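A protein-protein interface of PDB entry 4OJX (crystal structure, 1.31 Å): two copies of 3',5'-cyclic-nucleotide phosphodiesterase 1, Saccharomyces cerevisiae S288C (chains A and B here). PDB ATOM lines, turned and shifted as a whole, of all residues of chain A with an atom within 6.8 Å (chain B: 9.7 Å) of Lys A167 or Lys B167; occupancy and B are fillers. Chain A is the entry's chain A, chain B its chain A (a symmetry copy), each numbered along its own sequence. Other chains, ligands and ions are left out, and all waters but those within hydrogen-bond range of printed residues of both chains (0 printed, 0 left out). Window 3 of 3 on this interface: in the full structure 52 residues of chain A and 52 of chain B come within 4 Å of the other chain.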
ATOM      1  N   ILE A 162       3.227 -21.512 -16.503  1.00  0.00           N
ATOM      2  CA  ILE A 162       3.078 -20.079 -16.711  1.00  0.00           C
ATOM      3  C   ILE A 162       4.144 -19.260 -15.982  1.00  0.00           C
ATOM      4  O   ILE A 162       4.712 -18.321 -16.546  1.00  0.00           O
ATOM      5  CB  ILE A 162       1.652 -19.605 -16.353  1.00  0.00           C
ATOM      6  CG1 ILE A 162       0.621 -20.229 -17.310  1.00  0.00           C
ATOM      7  CG2 ILE A 162       1.565 -18.082 -16.363  1.00  0.00           C
ATOM      8  CD1 ILE A 162       0.807 -19.892 -18.778  1.00  0.00           C
ATOM      9  N   ASP A 163       4.429 -19.625 -14.736  1.00  0.00           N
ATOM     10  CA  ASP A 163       5.429 -18.904 -13.959  1.00  0.00           C
ATOM     11  C   ASP A 163       6.795 -18.970 -14.648  1.00  0.00           C
ATOM     12  O   ASP A 163       7.525 -17.978 -14.712  1.00  0.00           O
ATOM     13  CB  ASP A 163       5.517 -19.461 -12.532  1.00  0.00           C
ATOM     14  CG  ASP A 163       4.236 -19.262 -11.729  1.00  0.00           C
ATOM     15  OD1 ASP A 163       3.381 -18.437 -12.122  1.00  0.00           O
ATOM     16  OD2 ASP A 163       4.095 -19.939 -10.689  1.00  0.00           O
ATOM     17  N   VAL A 164       7.137 -20.141 -15.170  1.00  0.00           N
ATOM     18  CA  VAL A 164       8.412 -20.317 -15.852  1.00  0.00           C
ATOM     19  C   VAL A 164       8.455 -19.493 -17.139  1.00  0.00           C
ATOM     20  O   VAL A 164       9.459 -18.853 -17.432  1.00  0.00           O
ATOM     21  CB  VAL A 164       8.697 -21.807 -16.121  1.00  0.00           C
ATOM     22  CG1 VAL A 164       9.891 -21.979 -17.050  1.00  0.00           C
ATOM     23  CG2 VAL A 164       8.936 -22.540 -14.806  1.00  0.00           C
ATOM     24  N   LEU A 165       7.368 -19.484 -17.905  1.00  0.00           N
ATOM     25  CA  LEU A 165       7.344 -18.670 -19.123  1.00  0.00           C
ATOM     26  C   LEU A 165       7.530 -17.182 -18.809  1.00  0.00           C
ATOM     27  O   LEU A 165       8.263 -16.477 -19.514  1.00  0.00           O
ATOM     28  CB  LEU A 165       6.059 -18.897 -19.920  1.00  0.00           C
ATOM     29  CG  LEU A 165       5.872 -20.303 -20.492  1.00  0.00           C
ATOM     30  CD1 LEU A 165       4.561 -20.381 -21.254  1.00  0.00           C
ATOM     31  CD2 LEU A 165       7.035 -20.725 -21.381  1.00  0.00           C
ATOM     32  N   GLN A 166       6.884 -16.706 -17.744  1.00  0.00           N
ATOM     33  CA  GLN A 166       6.984 -15.304 -17.388  1.00  0.00           C
ATOM     34  C   GLN A 166       8.403 -14.944 -16.960  1.00  0.00           C
ATOM     35  O   GLN A 166       8.931 -13.921 -17.379  1.00  0.00           O
ATOM     36  CB  GLN A 166       5.992 -14.975 -16.274  1.00  0.00           C
ATOM     37  CG  GLN A 166       5.796 -13.485 -16.023  1.00  0.00           C
ATOM     38  CD  GLN A 166       4.835 -12.856 -17.012  1.00  0.00           C
ATOM     39  OE1 GLN A 166       3.645 -13.171 -17.025  1.00  0.00           O
ATOM     40  NE2 GLN A 166       5.343 -11.966 -17.843  1.00  0.00           N
ATOM     41  N   LYS A 167       9.015 -15.789 -16.134  1.00  0.00           N
ATOM     42  CA  LYS A 167      10.307 -15.478 -15.532  1.00  0.00           C
ATOM     43  C   LYS A 167      11.478 -15.734 -16.475  1.00  0.00           C
ATOM     44  O   LYS A 167      12.462 -14.999 -16.480  1.00  0.00           O
ATOM     45  CB  LYS A 167      10.492 -16.300 -14.247  1.00  0.00           C
ATOM     46  CG  LYS A 167      11.778 -16.018 -13.490  1.00  0.00           C
ATOM     47  CD  LYS A 167      11.738 -16.576 -12.075  1.00  0.00           C
ATOM     48  CE  LYS A 167      13.117 -16.549 -11.429  1.00  0.00           C
ATOM     49  NZ  LYS A 167      13.767 -15.209 -11.478  1.00  0.00           N
ATOM     50  N   HIS A 168      11.374 -16.802 -17.260  1.00  0.00           N
ATOM     51  CA  HIS A 168      12.528 -17.320 -17.994  1.00  0.00           C
ATOM     52  C   HIS A 168      12.484 -17.167 -19.482  1.00  0.00           C
ATOM     53  O   HIS A 168      13.509 -17.340 -20.127  1.00  0.00           O
ATOM     54  CB  HIS A 168      12.782 -18.769 -17.597  1.00  0.00           C
ATOM     55  CG  HIS A 168      13.121 -18.918 -16.147  1.00  0.00           C
ATOM     56  ND1 HIS A 168      14.222 -18.374 -15.623  1.00  0.00           N
ATOM     57  CD2 HIS A 168      12.454 -19.541 -15.107  1.00  0.00           C
ATOM     58  CE1 HIS A 168      14.269 -18.625 -14.314  1.00  0.00           C
ATOM     59  NE2 HIS A 168      13.191 -19.344 -13.993  1.00  0.00           N
ATOM     60  N   VAL A 169      11.320 -16.832 -20.034  1.00  0.00           N
ATOM     61  CA  VAL A 169      11.182 -16.697 -21.488  1.00  0.00           C
ATOM     62  C   VAL A 169      10.842 -15.268 -21.888  1.00  0.00           C
ATOM     63  O   VAL A 169      11.638 -14.605 -22.560  1.00  0.00           O
ATOM     64  CB  VAL A 169      10.153 -17.695 -22.064  1.00  0.00           C
ATOM     65  CG1 VAL A 169       9.976 -17.477 -23.562  1.00  0.00           C
ATOM     66  CG2 VAL A 169      10.598 -19.123 -21.789  1.00  0.00           C
ATOM     67  N   PHE A 170       9.665 -14.801 -21.477  1.00  0.00           N
ATOM     68  CA  PHE A 170       9.207 -13.466 -21.843  1.00  0.00           C
ATOM     69  C   PHE A 170       9.750 -12.467 -20.837  1.00  0.00           C
ATOM     70  O   PHE A 170       9.013 -11.895 -20.031  1.00  0.00           O
ATOM     71  CB  PHE A 170       7.684 -13.436 -21.942  1.00  0.00           C
ATOM     72  CG  PHE A 170       7.154 -14.345 -23.008  1.00  0.00           C
ATOM     73  CD1 PHE A 170       7.312 -14.030 -24.360  1.00  0.00           C
ATOM     74  CD2 PHE A 170       6.506 -15.529 -22.674  1.00  0.00           C
ATOM     75  CE1 PHE A 170       6.839 -14.883 -25.354  1.00  0.00           C
ATOM     76  CE2 PHE A 170       6.026 -16.376 -23.664  1.00  0.00           C
ATOM     77  CZ  PHE A 170       6.189 -16.058 -25.002  1.00  0.00           C
ATOM     78  N   ASN A 171      11.064 -12.257 -20.904  1.00  0.00           N
ATOM     79  CA  ASN A 171      11.793 -11.568 -19.845  1.00  0.00           C
ATOM     80  C   ASN A 171      12.838 -10.583 -20.372  1.00  0.00           C
ATOM     81  O   ASN A 171      13.717 -10.146 -19.628  1.00  0.00           O
ATOM     82  CB  ASN A 171      12.442 -12.583 -18.894  1.00  0.00           C
ATOM     83  CG  ASN A 171      13.509 -13.430 -19.569  1.00  0.00           C
ATOM     84  OD1 ASN A 171      13.854 -13.213 -20.737  1.00  0.00           O
ATOM     85  ND2 ASN A 171      14.052 -14.390 -18.831  1.00  0.00           N
ATOM     86  N   LEU A 173      15.309 -11.077 -22.095  1.00  0.00           N
ATOM     87  CA  LEU A 173      16.627 -11.704 -22.163  1.00  0.00           C
ATOM     88  C   LEU A 173      16.601 -12.875 -23.157  1.00  0.00           C
ATOM     89  O   LEU A 173      17.300 -12.872 -24.168  1.00  0.00           O
ATOM     90  CB  LEU A 173      17.070 -12.147 -20.764  1.00  0.00           C
ATOM     91  CG  LEU A 173      17.172 -11.028 -19.718  1.00  0.00           C
ATOM     92  CD1 LEU A 173      17.276 -11.607 -18.315  1.00  0.00           C
ATOM     93  CD2 LEU A 173      18.360 -10.118 -20.013  1.00  0.00           C
ATOM     94  N   LEU A 188      -0.545 -14.305 -20.925  1.00  0.00           N
ATOM     95  CA  LEU A 188      -0.335 -15.552 -20.192  1.00  0.00           C
ATOM     96  C   LEU A 188      -1.447 -15.714 -19.169  1.00  0.00           C
ATOM     97  O   LEU A 188      -1.717 -14.790 -18.397  1.00  0.00           O
ATOM     98  CB  LEU A 188       1.013 -15.541 -19.467  1.00  0.00           C
ATOM     99  CG  LEU A 188       2.299 -15.543 -20.297  1.00  0.00           C
ATOM    100  CD1 LEU A 188       3.498 -15.165 -19.447  1.00  0.00           C
ATOM    101  CD2 LEU A 188       2.549 -16.908 -20.906  1.00  0.00           C
ATOM    102  N   PRO B 129      21.422 -14.454 -26.398  1.00  0.00           N
ATOM    103  CA  PRO B 129      20.632 -15.606 -25.983  1.00  0.00           C
ATOM    104  C   PRO B 129      19.159 -15.577 -26.407  1.00  0.00           C
ATOM    105  O   PRO B 129      18.364 -16.347 -25.884  1.00  0.00           O
ATOM    106  CB  PRO B 129      20.786 -15.576 -24.464  1.00  0.00           C
ATOM    107  CG  PRO B 129      20.817 -14.104 -24.164  1.00  0.00           C
ATOM    108  CD  PRO B 129      21.620 -13.499 -25.285  1.00  0.00           C
ATOM    109  N   PRO B 159      29.668 -12.180 -21.292  1.00  0.00           N
ATOM    110  CA  PRO B 159      28.815 -12.349 -20.095  1.00  0.00           C
ATOM    111  C   PRO B 159      27.292 -12.148 -20.288  1.00  0.00           C
ATOM    112  O   PRO B 159      26.509 -12.920 -19.717  1.00  0.00           O
ATOM    113  CB  PRO B 159      29.392 -11.322 -19.122  1.00  0.00           C
ATOM    114  CG  PRO B 159      30.831 -11.237 -19.509  1.00  0.00           C
ATOM    115  CD  PRO B 159      30.857 -11.351 -21.009  1.00  0.00           C
ATOM    116  N   HIS B 160      26.859 -11.181 -21.100  1.00  0.00           N
ATOM    117  CA  HIS B 160      25.412 -10.936 -21.316  1.00  0.00           C
ATOM    118  C   HIS B 160      24.727 -12.132 -21.911  1.00  0.00           C
ATOM    119  O   HIS B 160      23.501 -12.261 -21.855  1.00  0.00           O
ATOM    120  CB  HIS B 160      25.170  -9.711 -22.203  1.00  0.00           C
ATOM    121  CG  HIS B 160      25.490  -9.934 -23.675  1.00  0.00           C
ATOM    122  ND1 HIS B 160      26.648  -9.526 -24.229  1.00  0.00           N
ATOM    123  CD2 HIS B 160      24.746 -10.535 -24.709  1.00  0.00           C
ATOM    124  CE1 HIS B 160      26.654  -9.830 -25.541  1.00  0.00           C
ATOM    125  NE2 HIS B 160      25.491 -10.460 -25.831  1.00  0.00           N
ATOM    126  N   THR B 161      25.524 -13.010 -22.503  1.00  0.00           N
ATOM    127  CA  THR B 161      25.017 -14.226 -23.103  1.00  0.00           C
ATOM    128  C   THR B 161      25.111 -15.399 -22.140  1.00  0.00           C
ATOM    129  O   THR B 161      24.111 -16.067 -21.877  1.00  0.00           O
ATOM    130  CB  THR B 161      25.787 -14.525 -24.389  1.00  0.00           C
ATOM    131  OG1 THR B 161      25.542 -13.472 -25.329  1.00  0.00           O
ATOM    132  CG2 THR B 161      25.351 -15.845 -24.982  1.00  0.00           C
ATOM    133  N   ILE B 162      26.297 -15.638 -21.594  1.00  0.00           N
ATOM    134  CA  ILE B 162      26.519 -16.800 -20.748  1.00  0.00           C
ATOM    135  C   ILE B 162      25.680 -16.771 -19.469  1.00  0.00           C
ATOM    136  O   ILE B 162      25.093 -17.783 -19.078  1.00  0.00           O
ATOM    137  CB  ILE B 162      28.020 -16.993 -20.439  1.00  0.00           C
ATOM    138  CG1 ILE B 162      28.797 -17.317 -21.727  1.00  0.00           C
ATOM    139  CG2 ILE B 162      28.226 -18.073 -19.382  1.00  0.00           C
ATOM    140  CD1 ILE B 162      28.364 -18.580 -22.449  1.00  0.00           C
ATOM    141  N   ASP B 163      25.609 -15.609 -18.828  1.00  0.00           N
ATOM    142  CA  ASP B 163      24.835 -15.482 -17.600  1.00  0.00           C
ATOM    143  C   ASP B 163      23.363 -15.815 -17.855  1.00  0.00           C
ATOM    144  O   ASP B 163      22.715 -16.496 -17.056  1.00  0.00           O
ATOM    145  CB  ASP B 163      24.975 -14.072 -17.010  1.00  0.00           C
ATOM    146  CG  ASP B 163      26.397 -13.745 -16.567  1.00  0.00           C
ATOM    147  OD1 ASP B 163      27.226 -14.670 -16.411  1.00  0.00           O
ATOM    148  OD2 ASP B 163      26.678 -12.545 -16.368  1.00  0.00           O
ATOM    149  N   VAL B 164      22.835 -15.338 -18.975  1.00  0.00           N
ATOM    150  CA  VAL B 164      21.444 -15.597 -19.321  1.00  0.00           C
ATOM    151  C   VAL B 164      21.223 -17.083 -19.602  1.00  0.00           C
ATOM    152  O   VAL B 164      20.237 -17.658 -19.156  1.00  0.00           O
ATOM    153  CB  VAL B 164      20.993 -14.721 -20.506  1.00  0.00           C
ATOM    154  CG1 VAL B 164      19.635 -15.164 -21.032  1.00  0.00           C
ATOM    155  CG2 VAL B 164      20.951 -13.256 -20.088  1.00  0.00           C
ATOM    156  N   LEU B 165      22.143 -17.720 -20.322  1.00  0.00           N
ATOM    157  CA  LEU B 165      21.999 -19.156 -20.575  1.00  0.00           C
ATOM    158  C   LEU B 165      21.997 -19.960 -19.272  1.00  0.00           C
ATOM    159  O   LEU B 165      21.202 -20.896 -19.110  1.00  0.00           O
ATOM    160  CB  LEU B 165      23.088 -19.666 -21.521  1.00  0.00           C
ATOM    161  CG  LEU B 165      23.049 -19.102 -22.942  1.00  0.00           C
ATOM    162  CD1 LEU B 165      24.181 -19.693 -23.764  1.00  0.00           C
ATOM    163  CD2 LEU B 165      21.708 -19.343 -23.624  1.00  0.00           C
ATOM    164  N   GLN B 166      22.869 -19.590 -18.334  1.00  0.00           N
ATOM    165  CA  GLN B 166      22.951 -20.311 -17.078  1.00  0.00           C
ATOM    166  C   GLN B 166      21.673 -20.145 -16.263  1.00  0.00           C
ATOM    167  O   GLN B 166      21.159 -21.116 -15.721  1.00  0.00           O
ATOM    168  CB  GLN B 166      24.160 -19.830 -16.277  1.00  0.00           C
ATOM    169  CG  GLN B 166      24.519 -20.712 -15.087  1.00  0.00           C
ATOM    170  CD  GLN B 166      25.322 -21.930 -15.495  1.00  0.00           C
ATOM    171  OE1 GLN B 166      26.458 -21.815 -15.952  1.00  0.00           O
ATOM    172  NE2 GLN B 166      24.738 -23.103 -15.330  1.00  0.00           N
ATOM    173  N   LYS B 167      21.164 -18.919 -16.186  1.00  0.00           N
ATOM    174  CA  LYS B 167      20.038 -18.605 -15.311  1.00  0.00           C
ATOM    175  C   LYS B 167      18.693 -19.002 -15.910  1.00  0.00           C
ATOM    176  O   LYS B 167      17.788 -19.440 -15.206  1.00  0.00           O
ATOM    177  CB  LYS B 167      20.035 -17.104 -14.987  1.00  0.00           C
ATOM    178  CG  LYS B 167      18.943 -16.661 -14.029  1.00  0.00           C
ATOM    179  CD  LYS B 167      19.206 -15.270 -13.472  1.00  0.00           C
ATOM    180  CE  LYS B 167      17.981 -14.719 -12.752  1.00  0.00           C
ATOM    181  NZ  LYS B 167      17.444 -15.640 -11.711  1.00  0.00           N
ATOM    182  N   HIS B 168      18.560 -18.819 -17.220  1.00  0.00           N
ATOM    183  CA  HIS B 168      17.250 -18.884 -17.867  1.00  0.00           C
ATOM    184  C   HIS B 168      17.022 -20.050 -18.776  1.00  0.00           C
ATOM    185  O   HIS B 168      15.883 -20.304 -19.143  1.00  0.00           O
ATOM    186  CB  HIS B 168      16.960 -17.568 -18.578  1.00  0.00           C
ATOM    187  CG  HIS B 168      16.892 -16.408 -17.635  1.00  0.00           C
ATOM    188  ND1 HIS B 168      15.958 -16.328 -16.684  1.00  0.00           N
ATOM    189  CD2 HIS B 168      17.692 -15.287 -17.497  1.00  0.00           C
ATOM    190  CE1 HIS B 168      16.140 -15.220 -15.965  1.00  0.00           C
ATOM    191  NE2 HIS B 168      17.198 -14.575 -16.462  1.00  0.00           N
ATOM    192  N   VAL B 169      18.083 -20.770 -19.135  1.00  0.00           N
ATOM    193  CA  VAL B 169      17.953 -21.907 -20.052  1.00  0.00           C
ATOM    194  C   VAL B 169      18.325 -23.219 -19.374  1.00  0.00           C
ATOM    195  O   VAL B 169      17.471 -24.096 -19.209  1.00  0.00           O
ATOM    196  CB  VAL B 169      18.771 -21.700 -21.346  1.00  0.00           C
ATOM    197  CG1 VAL B 169      18.677 -22.929 -22.242  1.00  0.00           C
ATOM    198  CG2 VAL B 169      18.273 -20.469 -22.088  1.00  0.00           C
ATOM    199  N   PHE B 170      19.592 -23.349 -18.987  1.00  0.00           N
ATOM    200  CA  PHE B 170      20.077 -24.579 -18.376  1.00  0.00           C
ATOM    201  C   PHE B 170      19.817 -24.521 -16.881  1.00  0.00           C
ATOM    202  O   PHE B 170      20.738 -24.410 -16.069  1.00  0.00           O
ATOM    203  CB  PHE B 170      21.552 -24.793 -18.711  1.00  0.00           C
ATOM    204  CG  PHE B 170      21.795 -24.956 -20.180  1.00  0.00           C
ATOM    205  CD1 PHE B 170      21.409 -26.122 -20.845  1.00  0.00           C
ATOM    206  CD2 PHE B 170      22.397 -23.942 -20.916  1.00  0.00           C
ATOM    207  CE1 PHE B 170      21.615 -26.268 -22.214  1.00  0.00           C
ATOM    208  CE2 PHE B 170      22.611 -24.090 -22.280  1.00  0.00           C
ATOM    209  CZ  PHE B 170      22.223 -25.248 -22.931  1.00  0.00           C
ATOM    210  N   ASN B 171      18.536 -24.611 -16.528  1.00  0.00           N
ATOM    211  CA  ASN B 171      18.079 -24.284 -15.182  1.00  0.00           C
ATOM    212  C   ASN B 171      17.035 -25.264 -14.643  1.00  0.00           C
ATOM    213  O   ASN B 171      16.351 -24.971 -13.661  1.00  0.00           O
ATOM    214  CB  ASN B 171      17.543 -22.846 -15.134  1.00  0.00           C
ATOM    215  CG  ASN B 171      16.303 -22.647 -15.990  1.00  0.00           C
ATOM    216  OD1 ASN B 171      15.761 -23.599 -16.563  1.00  0.00           O
ATOM    217  ND2 ASN B 171      15.834 -21.408 -16.067  1.00  0.00           N
ATOM    218  N   ASP B 172      16.918 -26.429 -15.281  1.00  0.00           N
ATOM    219  CA  ASP B 172      15.960 -27.468 -14.876  1.00  0.00           C
ATOM    220  C   ASP B 172      14.490 -27.059 -15.010  1.00  0.00           C
ATOM    221  O   ASP B 172      13.588 -27.769 -14.552  1.00  0.00           O
ATOM    222  CB  ASP B 172      16.291 -28.002 -13.476  1.00  0.00           C
ATOM    223  CG  ASP B 172      17.579 -28.783 -13.456  1.00  0.00           C
ATOM    224  OD1 ASP B 172      17.803 -29.579 -14.396  1.00  0.00           O
ATOM    225  OD2 ASP B 172      18.352 -28.643 -12.485  1.00  0.00           O
ATOM    226  N   LEU B 173      14.251 -25.942 -15.693  1.00  0.00           N
ATOM    227  CA  LEU B 173      12.898 -25.445 -15.934  1.00  0.00           C
ATOM    228  C   LEU B 173      12.640 -25.333 -17.444  1.00  0.00           C
ATOM    229  O   LEU B 173      11.765 -25.996 -17.995  1.00  0.00           O
ATOM    230  CB  LEU B 173      12.695 -24.107 -15.215  1.00  0.00           C
ATOM    231  CG  LEU B 173      12.883 -24.140 -13.692  1.00  0.00           C
ATOM    232  CD1 LEU B 173      13.001 -22.732 -13.130  1.00  0.00           C
ATOM    233  CD2 LEU B 173      11.737 -24.892 -13.021  1.00  0.00           C
ATOM    234  N   ILE B 174      13.450 -24.523 -18.119  1.00  0.00           N
ATOM    235  CA  ILE B 174      13.406 -24.407 -19.575  1.00  0.00           C
ATOM    236  C   ILE B 174      14.105 -25.594 -20.244  1.00  0.00           C
ATOM    237  O   ILE B 174      13.715 -26.041 -21.321  1.00  0.00           O
ATOM    238  CB  ILE B 174      14.002 -23.052 -20.017  1.00  0.00           C
ATOM    239  CG1 ILE B 174      13.092 -21.910 -19.553  1.00  0.00           C
ATOM    240  CG2 ILE B 174      14.243 -23.009 -21.522  1.00  0.00           C
ATOM    241  CD1 ILE B 174      11.690 -21.950 -20.125  1.00  0.00           C
ATOM    242  N   TRP B 175      15.135 -26.109 -19.587  1.00  0.00           N
ATOM    243  CA  TRP B 175      15.878 -27.254 -20.080  1.00  0.00           C
ATOM    244  C   TRP B 175      16.552 -27.900 -18.911  1.00  0.00           C
ATOM    245  O   TRP B 175      16.974 -27.194 -17.993  1.00  0.00           O
ATOM    246  CB  TRP B 175      16.941 -26.827 -21.090  1.00  0.00           C
ATOM    247  CG  TRP B 175      17.334 -27.952 -22.004  1.00  0.00           C
ATOM    248  CD1 TRP B 175      18.568 -28.570 -22.119  1.00  0.00           C
ATOM    249  CD2 TRP B 175      16.468 -28.620 -22.964  1.00  0.00           C
ATOM    250  NE1 TRP B 175      18.526 -29.563 -23.068  1.00  0.00           N
ATOM    251  CE2 TRP B 175      17.278 -29.643 -23.610  1.00  0.00           C
ATOM    252  CE3 TRP B 175      15.134 -28.483 -23.322  1.00  0.00           C
ATOM    253  CZ2 TRP B 175      16.765 -30.456 -24.605  1.00  0.00           C
ATOM    254  CZ3 TRP B 175      14.620 -29.325 -24.312  1.00  0.00           C
ATOM    255  CH2 TRP B 175      15.420 -30.286 -24.940  1.00  0.00           C
ATOM    256  N   ASP B 177      19.412 -29.002 -16.626  1.00  0.00           N
ATOM    257  CA  ASP B 177      20.674 -28.305 -16.494  1.00  0.00           C
ATOM    258  C   ASP B 177      21.828 -29.257 -16.791  1.00  0.00           C
ATOM    259  O   ASP B 177      22.472 -29.800 -15.892  1.00  0.00           O
ATOM    260  CB  ASP B 177      20.822 -27.652 -15.119  1.00  0.00           C
ATOM    261  CG  ASP B 177      22.108 -26.863 -15.004  1.00  0.00           C
ATOM    262  OD1 ASP B 177      22.899 -26.863 -15.985  1.00  0.00           O
ATOM    263  OD2 ASP B 177      22.309 -26.244 -13.929  1.00  0.00           O
ATOM    264  N   THR B 179      24.685 -28.642 -17.800  1.00  0.00           N
ATOM    265  CA  THR B 179      25.990 -28.166 -17.331  1.00  0.00           C
ATOM    266  C   THR B 179      26.326 -28.679 -15.923  1.00  0.00           C
ATOM    267  O   THR B 179      27.489 -28.678 -15.527  1.00  0.00           O
ATOM    268  CB  THR B 179      26.125 -26.631 -17.387  1.00  0.00           C
ATOM    269  OG1 THR B 179      25.415 -26.035 -16.291  1.00  0.00           O
ATOM    270  CG2 THR B 179      25.609 -26.099 -18.720  1.00  0.00           C
ATOM    271  N   LEU B 188      29.727 -24.124 -20.199  1.00  0.00           N
ATOM    272  CA  LEU B 188      29.561 -22.714 -20.547  1.00  0.00           C
ATOM    273  C   LEU B 188      30.830 -21.963 -20.178  1.00  0.00           C
ATOM    274  O   LEU B 188      31.315 -22.085 -19.050  1.00  0.00           O
ATOM    275  CB  LEU B 188      28.381 -22.099 -19.791  1.00  0.00           C
ATOM    276  CG  LEU B 188      26.964 -22.583 -20.111  1.00  0.00           C
ATOM    277  CD1 LEU B 188      25.983 -22.148 -19.039  1.00  0.00           C
ATOM    278  CD2 LEU B 188      26.494 -22.040 -21.446  1.00  0.00           C
ATOM    279  N   LYS B 218       9.746  -4.493 -21.408  1.00  0.00           N
ATOM    280  CA  LYS B 218       9.319  -4.132 -20.062  1.00  0.00           C
ATOM    281  C   LYS B 218      10.378  -3.295 -19.377  1.00  0.00           C
ATOM    282  O   LYS B 218      10.064  -2.302 -18.728  1.00  0.00           O
ATOM    283  CB  LYS B 218       9.029  -5.385 -19.227  1.00  0.00           C
ATOM    284  CG  LYS B 218       8.337  -5.098 -17.899  1.00  0.00           C
ATOM    285  CD  LYS B 218       8.080  -6.377 -17.120  1.00  0.00           C
ATOM    286  CE  LYS B 218       7.145  -6.138 -15.946  1.00  0.00           C
ATOM    287  NZ  LYS B 218       7.743  -5.191 -14.968  1.00  0.00           N
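A ring nitrogen (ND1) of His A168 lies within hydrogen-bond range of a ring nitrogen (ND1) of His B168, at 2.9 Å.
A ring nitrogen (ND1) of His A168 lies within hydrogen-bond range of the side-chain amide nitrogen (ND2) of Asn B171, 3.5 Å away.
ND1 of His B168 sits at hydrogen-bond distance from ND2 of Asn A171.
OD1 of Asn A171 is in hydrogen-bond range of N of Leu A173.
The backbone carbonyl oxygen (O) of Lys B167 is in hydrogen-bond range of the side-chain amide nitrogen (ND2) of Asn B171 (2.9 Å).
The side-chain amide nitrogen of Asn B171 lies close to the backbone carbonyl oxygen of His B168 (3.3 Å).
The backbone carbonyl oxygen of Val B169 sits close to the side-chain amide oxygen of Asn B171 (3.2 Å).
The backbone NH (N) of Leu B173 is in hydrogen-bond range of the side-chain amide oxygen (OD1) of Asn B171, 2.9 Å away.
The side-chain amide oxygen (OD1) of Asn B171 is in hydrogen-bond range of the backbone NH (N) of Ile B174 (2.9 Å).
Val A164 touches Leu B173.
Lys B167 touches Lys A167.
His B168 touches Lys A167.
His A168 touches Lys B167 (CE1 to O, 3.7 Å).
His A168 touches Leu B173 (NE2 to CD1, 3.5 Å).
CB of His A168 touches CG1 of Ile B174, 3.7 Å away.
CD1 of Ile B174 touches CG2 of Val A169, at 3.5 Å.
Leu A173 touches Pro B129.
CB of Leu A173 touches CG1 of Val B164 (3.97 Å).
Leu A173 touches His B168 (CD1 to NE2, 3.5 Å).
Lys A167 touches just these residues of chain B: Lys B167 and His B168.
Lys B167 touches just these residues of chain A: Lys A167 (3.7 Å) and His A168 (3.7 Å).
Of chain B, only Lys B167 (3.7 Å), His B168 (2.9 Å), Asn B171 (3.5 Å), Leu B173 (3.5 Å) and Ile B174 (3.7 Å) come within 4 Å of His A168.
Of the printed residues of chain A, Asn B171 touches His A168.
Printed residues of chain A within 4 Å of Pro B129: Leu A173.
Of the printed residues of chain B, Asn A171 touches His B168.
Of the printed residues of chain A, Val B164 touches Leu A173.
Printed residues of chain A within 4 Å of Ile B174: Val A164, His A168 and Val A169.
Pro B159 touches none of the printed residues of chain A.
Printed residues of chain A that touch a printed residue of chain B: Val A164, Lys A167, His A168, Val A169, Asn A171 and Leu A173.
Hydrophobic or aromatic side chains of chain A within 4 Å of the printed part of chain B: Val A164, His A168, Val A169 and Leu A173.
Along chain A the printed residues that touch a printed residue of chain B span positions 164 to 173.
Val A164 touches Leu B173, and with the chains exchanged Leu A173 touches Val B164.
Lys A167 touches His B168, and with the chains exchanged His A168 touches Lys B167.
His B168 touches its own counterpart, His A168.
His A168 touches Leu B173, and with the chains exchanged Leu A173 touches His B168.
Positions printed for both chains: 162, 163, 164, 165, 166, 167, 168, 169, 170, 171, 173 and 188.
Of the 14 pairs that touch across the chains among the printed residues, 10 have their exchanged pair printed and touching as well.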
